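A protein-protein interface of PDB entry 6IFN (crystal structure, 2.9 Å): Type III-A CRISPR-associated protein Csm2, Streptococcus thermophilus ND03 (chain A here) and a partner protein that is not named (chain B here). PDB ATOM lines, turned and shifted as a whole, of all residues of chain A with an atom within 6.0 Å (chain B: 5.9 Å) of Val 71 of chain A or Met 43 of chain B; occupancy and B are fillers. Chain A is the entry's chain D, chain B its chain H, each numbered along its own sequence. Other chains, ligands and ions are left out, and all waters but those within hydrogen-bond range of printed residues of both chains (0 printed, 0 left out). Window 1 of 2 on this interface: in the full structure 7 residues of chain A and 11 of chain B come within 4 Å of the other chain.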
ATOM      1  N   ILE A  66       7.451  11.882   1.300  1.00  0.00           N
ATOM      2  CA  ILE A  66       8.612  12.189   2.144  1.00  0.00           C
ATOM      3  C   ILE A  66       8.655  13.690   2.466  1.00  0.00           C
ATOM      4  O   ILE A  66       9.117  14.076   3.541  1.00  0.00           O
ATOM      5  CB  ILE A  66       9.921  11.682   1.504  1.00  0.00           C
ATOM      6  CG1 ILE A  66       9.916  10.154   1.435  1.00  0.00           C
ATOM      7  CG2 ILE A  66      11.152  12.199   2.243  1.00  0.00           C
ATOM      8  CD1 ILE A  66       9.429   9.589   0.129  1.00  0.00           C
ATOM      9  N   ALA A  67       8.197  14.528   1.528  1.00  0.00           N
ATOM     10  CA  ALA A  67       7.970  15.944   1.828  1.00  0.00           C
ATOM     11  C   ALA A  67       6.966  16.049   2.977  1.00  0.00           C
ATOM     12  O   ALA A  67       7.286  16.589   4.007  1.00  0.00           O
ATOM     13  CB  ALA A  67       7.500  16.699   0.609  1.00  0.00           C
ATOM     14  N   TYR A  68       5.769  15.474   2.786  1.00  0.00           N
ATOM     15  CA  TYR A  68       4.675  15.452   3.785  1.00  0.00           C
ATOM     16  C   TYR A  68       5.214  14.999   5.149  1.00  0.00           C
ATOM     17  O   TYR A  68       4.820  15.546   6.161  1.00  0.00           O
ATOM     18  CB  TYR A  68       3.542  14.540   3.305  1.00  0.00           C
ATOM     19  CG  TYR A  68       2.151  14.753   3.859  1.00  0.00           C
ATOM     20  CD1 TYR A  68       1.906  14.937   5.210  1.00  0.00           C
ATOM     21  CD2 TYR A  68       1.047  14.646   3.018  1.00  0.00           C
ATOM     22  CE1 TYR A  68       0.611  15.072   5.696  1.00  0.00           C
ATOM     23  CE2 TYR A  68      -0.253  14.771   3.486  1.00  0.00           C
ATOM     24  CZ  TYR A  68      -0.469  14.994   4.832  1.00  0.00           C
ATOM     25  OH  TYR A  68      -1.741  15.142   5.295  1.00  0.00           O
ATOM     26  N   LEU A  69       6.110  14.003   5.168  1.00  0.00           N
ATOM     27  CA  LEU A  69       6.690  13.514   6.436  1.00  0.00           C
ATOM     28  C   LEU A  69       7.520  14.633   7.080  1.00  0.00           C
ATOM     29  O   LEU A  69       7.290  15.005   8.217  1.00  0.00           O
ATOM     30  CB  LEU A  69       7.497  12.254   6.223  1.00  0.00           C
ATOM     31  N   ARG A  70       8.460  15.202   6.331  1.00  0.00           N
ATOM     32  CA  ARG A  70       9.279  16.306   6.838  1.00  0.00           C
ATOM     33  C   ARG A  70       8.361  17.427   7.348  1.00  0.00           C
ATOM     34  O   ARG A  70       8.591  17.979   8.411  1.00  0.00           O
ATOM     35  CB  ARG A  70      10.211  16.822   5.735  1.00  0.00           C
ATOM     36  CG  ARG A  70      11.269  17.801   6.218  1.00  0.00           C
ATOM     37  CD  ARG A  70      12.466  17.949   5.280  1.00  0.00           C
ATOM     38  NE  ARG A  70      13.522  18.751   5.898  1.00  0.00           N
ATOM     39  CZ  ARG A  70      14.757  18.325   6.182  1.00  0.00           C
ATOM     40  NH1 ARG A  70      15.217  17.204   5.651  1.00  0.00           N
ATOM     41  NH2 ARG A  70      15.527  19.025   6.999  1.00  0.00           N
ATOM     42  N   VAL A  71       7.324  17.749   6.565  1.00  0.00           N
ATOM     43  CA  VAL A  71       6.397  18.827   6.878  1.00  0.00           C
ATOM     44  C   VAL A  71       5.837  18.593   8.285  1.00  0.00           C
ATOM     45  O   VAL A  71       6.054  19.422   9.183  1.00  0.00           O
ATOM     46  CB  VAL A  71       5.275  18.947   5.824  1.00  0.00           C
ATOM     47  CG1 VAL A  71       4.033  19.647   6.358  1.00  0.00           C
ATOM     48  CG2 VAL A  71       5.751  19.656   4.573  1.00  0.00           C
ATOM     49  N   GLN A  72       5.108  17.481   8.458  1.00  0.00           N
ATOM     50  CA  GLN A  72       4.445  17.198   9.725  1.00  0.00           C
ATOM     51  C   GLN A  72       5.491  17.094  10.841  1.00  0.00           C
ATOM     52  O   GLN A  72       5.196  17.417  11.978  1.00  0.00           O
ATOM     53  CB  GLN A  72       3.533  15.975   9.642  1.00  0.00           C
ATOM     54  CG  GLN A  72       2.069  16.351   9.485  1.00  0.00           C
ATOM     55  CD  GLN A  72       1.800  16.968   8.133  1.00  0.00           C
ATOM     56  OE1 GLN A  72       2.656  17.007   7.250  1.00  0.00           O
ATOM     57  NE2 GLN A  72       0.577  17.434   7.948  1.00  0.00           N
ATOM     58  N   PHE A  73       6.717  16.675  10.526  1.00  0.00           N
ATOM     59  CA  PHE A  73       7.790  16.708  11.522  1.00  0.00           C
ATOM     60  C   PHE A  73       7.933  18.140  12.049  1.00  0.00           C
ATOM     61  O   PHE A  73       7.874  18.370  13.243  1.00  0.00           O
ATOM     62  CB  PHE A  73       9.104  16.142  10.967  1.00  0.00           C
ATOM     63  CG  PHE A  73       9.283  14.666  11.230  1.00  0.00           C
ATOM     64  CD1 PHE A  73       9.655  14.222  12.489  1.00  0.00           C
ATOM     65  CD2 PHE A  73       9.031  13.716  10.242  1.00  0.00           C
ATOM     66  CE1 PHE A  73       9.804  12.870  12.745  1.00  0.00           C
ATOM     67  CE2 PHE A  73       9.160  12.362  10.501  1.00  0.00           C
ATOM     68  CZ  PHE A  73       9.558  11.945  11.751  1.00  0.00           C
ATOM     69  N   VAL A  74       8.105  19.100  11.140  1.00  0.00           N
ATOM     70  CA  VAL A  74       8.341  20.490  11.524  1.00  0.00           C
ATOM     71  C   VAL A  74       7.082  21.039  12.221  1.00  0.00           C
ATOM     72  O   VAL A  74       7.175  21.614  13.302  1.00  0.00           O
ATOM     73  CB  VAL A  74       8.773  21.347  10.315  1.00  0.00           C
ATOM     74  CG1 VAL A  74       9.295  22.697  10.770  1.00  0.00           C
ATOM     75  CG2 VAL A  74       9.811  20.652   9.438  1.00  0.00           C
ATOM     76  N   TYR A  75       5.906  20.857  11.603  1.00  0.00           N
ATOM     77  CA  TYR A  75       4.632  21.339  12.152  1.00  0.00           C
ATOM     78  C   TYR A  75       4.502  20.896  13.612  1.00  0.00           C
ATOM     79  O   TYR A  75       4.318  21.715  14.509  1.00  0.00           O
ATOM     80  CB  TYR A  75       3.476  20.801  11.310  1.00  0.00           C
ATOM     81  CG  TYR A  75       2.095  21.333  11.604  1.00  0.00           C
ATOM     82  CD1 TYR A  75       1.462  21.151  12.827  1.00  0.00           C
ATOM     83  CD2 TYR A  75       1.357  21.921  10.586  1.00  0.00           C
ATOM     84  CE1 TYR A  75       0.169  21.613  13.049  1.00  0.00           C
ATOM     85  CE2 TYR A  75       0.061  22.374  10.784  1.00  0.00           C
ATOM     86  CZ  TYR A  75      -0.540  22.221  12.020  1.00  0.00           C
ATOM     87  OH  TYR A  75      -1.816  22.692  12.163  1.00  0.00           O
ATOM     88  N   GLN A  76       4.621  19.582  13.830  1.00  0.00           N
ATOM     89  CA  GLN A  76       4.508  18.999  15.158  1.00  0.00           C
ATOM     90  C   GLN A  76       5.656  19.470  16.044  1.00  0.00           C
ATOM     91  O   GLN A  76       5.481  19.530  17.243  1.00  0.00           O
ATOM     92  CB  GLN A  76       4.478  17.469  15.100  1.00  0.00           C
ATOM     93  CG  GLN A  76       3.124  16.942  14.642  1.00  0.00           C
ATOM     94  CD  GLN A  76       2.043  17.440  15.565  1.00  0.00           C
ATOM     95  OE1 GLN A  76       2.278  17.599  16.761  1.00  0.00           O
ATOM     96  NE2 GLN A  76       0.873  17.724  15.011  1.00  0.00           N
ATOM     97  N   PRO B  41      -4.880  25.059   3.605  1.00  0.00           N
ATOM     98  CA  PRO B  41      -4.068  24.406   2.588  1.00  0.00           C
ATOM     99  C   PRO B  41      -3.844  22.924   2.921  1.00  0.00           C
ATOM    100  O   PRO B  41      -4.294  22.429   3.962  1.00  0.00           O
ATOM    101  CB  PRO B  41      -2.766  25.223   2.655  1.00  0.00           C
ATOM    102  CG  PRO B  41      -2.626  25.533   4.124  1.00  0.00           C
ATOM    103  CD  PRO B  41      -4.051  25.728   4.621  1.00  0.00           C
ATOM    104  N   ASP B  42      -3.144  22.233   2.018  1.00  0.00           N
ATOM    105  CA  ASP B  42      -2.568  20.958   2.304  1.00  0.00           C
ATOM    106  C   ASP B  42      -1.094  21.223   2.601  1.00  0.00           C
ATOM    107  O   ASP B  42      -0.353  21.561   1.684  1.00  0.00           O
ATOM    108  CB  ASP B  42      -2.793  19.990   1.147  1.00  0.00           C
ATOM    109  CG  ASP B  42      -2.375  18.575   1.489  1.00  0.00           C
ATOM    110  OD1 ASP B  42      -2.140  18.307   2.675  1.00  0.00           O
ATOM    111  OD2 ASP B  42      -2.284  17.755   0.574  1.00  0.00           O
ATOM    112  N   MET B  43      -0.711  21.122   3.883  1.00  0.00           N
ATOM    113  CA  MET B  43       0.656  21.423   4.347  1.00  0.00           C
ATOM    114  C   MET B  43       1.684  20.758   3.404  1.00  0.00           C
ATOM    115  O   MET B  43       2.708  21.369   3.078  1.00  0.00           O
ATOM    116  CB  MET B  43       0.872  20.978   5.801  1.00  0.00           C
ATOM    117  N   GLY B  44       1.387  19.536   2.928  1.00  0.00           N
ATOM    118  CA  GLY B  44       2.146  18.857   1.865  1.00  0.00           C
ATOM    119  C   GLY B  44       2.324  19.734   0.630  1.00  0.00           C
ATOM    120  O   GLY B  44       3.456  20.180   0.303  1.00  0.00           O
ATOM    121  N   LYS B  45       1.206  19.999  -0.057  1.00  0.00           N
ATOM    122  CA  LYS B  45       1.216  20.734  -1.334  1.00  0.00           C
ATOM    123  C   LYS B  45       1.908  22.095  -1.157  1.00  0.00           C
ATOM    124  O   LYS B  45       2.647  22.527  -2.052  1.00  0.00           O
ATOM    125  CB  LYS B  45      -0.197  20.916  -1.899  1.00  0.00           C
ATOM    126  CG  LYS B  45      -0.823  19.663  -2.502  1.00  0.00           C
ATOM    127  CD  LYS B  45      -1.239  19.794  -3.957  1.00  0.00           C
ATOM    128  CE  LYS B  45      -0.097  19.533  -4.919  1.00  0.00           C
ATOM    129  NZ  LYS B  45      -0.386  20.049  -6.277  1.00  0.00           N
ATOM    130  N   PHE B  46       1.660  22.759  -0.015  1.00  0.00           N
ATOM    131  CA  PHE B  46       2.397  23.969   0.369  1.00  0.00           C
ATOM    132  C   PHE B  46       3.889  23.685   0.249  1.00  0.00           C
ATOM    133  O   PHE B  46       4.574  24.376  -0.487  1.00  0.00           O
ATOM    134  CB  PHE B  46       2.084  24.436   1.794  1.00  0.00           C
ATOM    135  N   TYR B  47       4.353  22.637   0.941  1.00  0.00           N
ATOM    136  CA  TYR B  47       5.781  22.372   1.053  1.00  0.00           C
ATOM    137  C   TYR B  47       6.411  22.211  -0.333  1.00  0.00           C
ATOM    138  O   TYR B  47       7.513  22.712  -0.575  1.00  0.00           O
ATOM    139  CB  TYR B  47       6.088  21.132   1.893  1.00  0.00           C
ATOM    140  CG  TYR B  47       7.536  21.069   2.309  1.00  0.00           C
ATOM    141  CD1 TYR B  47       8.036  21.944   3.264  1.00  0.00           C
ATOM    142  CD2 TYR B  47       8.424  20.185   1.711  1.00  0.00           C
ATOM    143  CE1 TYR B  47       9.367  21.919   3.648  1.00  0.00           C
ATOM    144  CE2 TYR B  47       9.762  20.152   2.079  1.00  0.00           C
ATOM    145  CZ  TYR B  47      10.234  21.025   3.047  1.00  0.00           C
ATOM    146  OH  TYR B  47      11.545  21.013   3.411  1.00  0.00           O
ATOM    147  N   ASN B  48       5.699  21.527  -1.233  1.00  0.00           N
ATOM    148  CA  ASN B  48       6.267  21.112  -2.504  1.00  0.00           C
ATOM    149  C   ASN B  48       6.154  22.234  -3.549  1.00  0.00           C
ATOM    150  O   ASN B  48       6.890  22.218  -4.520  1.00  0.00           O
ATOM    151  CB  ASN B  48       5.680  19.761  -2.916  1.00  0.00           C
ATOM    152  CG  ASN B  48       6.174  18.666  -1.991  1.00  0.00           C
ATOM    153  OD1 ASN B  48       5.450  18.226  -1.101  1.00  0.00           O
ATOM    154  ND2 ASN B  48       7.433  18.278  -2.144  1.00  0.00           N
ATOM    155  N   PHE B  59      10.369  28.245   5.165  1.00  0.00           N
ATOM    156  CA  PHE B  59       9.088  27.691   5.651  1.00  0.00           C
ATOM    157  C   PHE B  59       9.341  26.823   6.879  1.00  0.00           C
ATOM    158  O   PHE B  59       8.615  26.926   7.844  1.00  0.00           O
ATOM    159  CB  PHE B  59       8.361  26.845   4.597  1.00  0.00           C
ATOM    160  CG  PHE B  59       6.855  26.796   4.746  1.00  0.00           C
ATOM    161  CD1 PHE B  59       6.257  26.520   5.969  1.00  0.00           C
ATOM    162  CD2 PHE B  59       6.028  27.024   3.650  1.00  0.00           C
ATOM    163  CE1 PHE B  59       4.876  26.495   6.090  1.00  0.00           C
ATOM    164  CE2 PHE B  59       4.645  26.983   3.770  1.00  0.00           C
ATOM    165  CZ  PHE B  59       4.074  26.722   4.993  1.00  0.00           C
ATOM    166  N   LEU B  63       8.225  27.355  10.651  1.00  0.00           N
ATOM    167  CA  LEU B  63       7.345  26.408  11.318  1.00  0.00           C
ATOM    168  C   LEU B  63       8.045  25.866  12.568  1.00  0.00           C
ATOM    169  O   LEU B  63       7.473  25.880  13.614  1.00  0.00           O
ATOM    170  CB  LEU B  63       6.948  25.295  10.343  1.00  0.00           C
ATOM    171  CG  LEU B  63       5.455  24.970  10.266  1.00  0.00           C
ATOM    172  CD1 LEU B  63       4.651  26.191   9.862  1.00  0.00           C
ATOM    173  CD2 LEU B  63       5.190  23.826   9.292  1.00  0.00           C
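The backbone carbonyl oxygen (O) of Gly 44 of chain B lies close to the side-chain amide oxygen (OD1) of Asn 48 of chain B.
Among the printed residues, merely in contact across the chains: Ala 67 of chain A with Tyr 47 of chain B, Ala 67 of chain A with Asn 48 of chain B, Arg 70 of chain A with Tyr 47 of chain B, Val 71 of chain A with Met 43 of chain B, Val 71 of chain A with Tyr 47 of chain B, Val 74 of chain A with Leu 63 of chain B and Tyr 75 of chain A with Leu 63 of chain B.
Met 43 of chain B touches just one residue of chain A: Val 71 (3.5 Å).
Of the printed residues of chain A, Tyr 47 of chain B touches Ala 67, Arg 70 and Val 71.
Printed residues of chain B within 4 Å of Val 74 of chain A: Leu 63.
Of the printed residues of chain A, Leu 63 of chain B touches Val 74 (3.5 Å) and Tyr 75 (3.8 Å).
Printed residues of chain B within 4 Å of Tyr 75 of chain A: Leu 63.
Of the printed residues of chain B, Ala 67 of chain A touches Tyr 47 and Asn 48.
The nearest residue of chain A that does not touch Met 43 of chain B is Gln 72 of chain A (4.2 Å).
The nearest printed residue of chain B that does not touch Val 74 of chain A is Phe 59 of chain B (5.2 Å).
Of the 11 printed residues of chain A, 5 touch a printed residue of chain B.
Printed residues of chain A that touch a printed residue of chain B: Ala 67, Arg 70, Val 71, Val 74 and Tyr 75.
Hydrophobic or aromatic side chains of chain A within 4 Å of the printed part of chain B: Ala 67, Val 71 and Val 74.
Of the 10 printed residues of chain B, 4 touch a printed residue of chain A.
Printed residues of chain B that touch a printed residue of chain A: Met 43, Tyr 47, Asn 48 and Leu 63.
Among the printed residues, no Asp or Glu carboxylate lies within 4 Å of a Lys or Arg side-chain nitrogen of the other chain.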
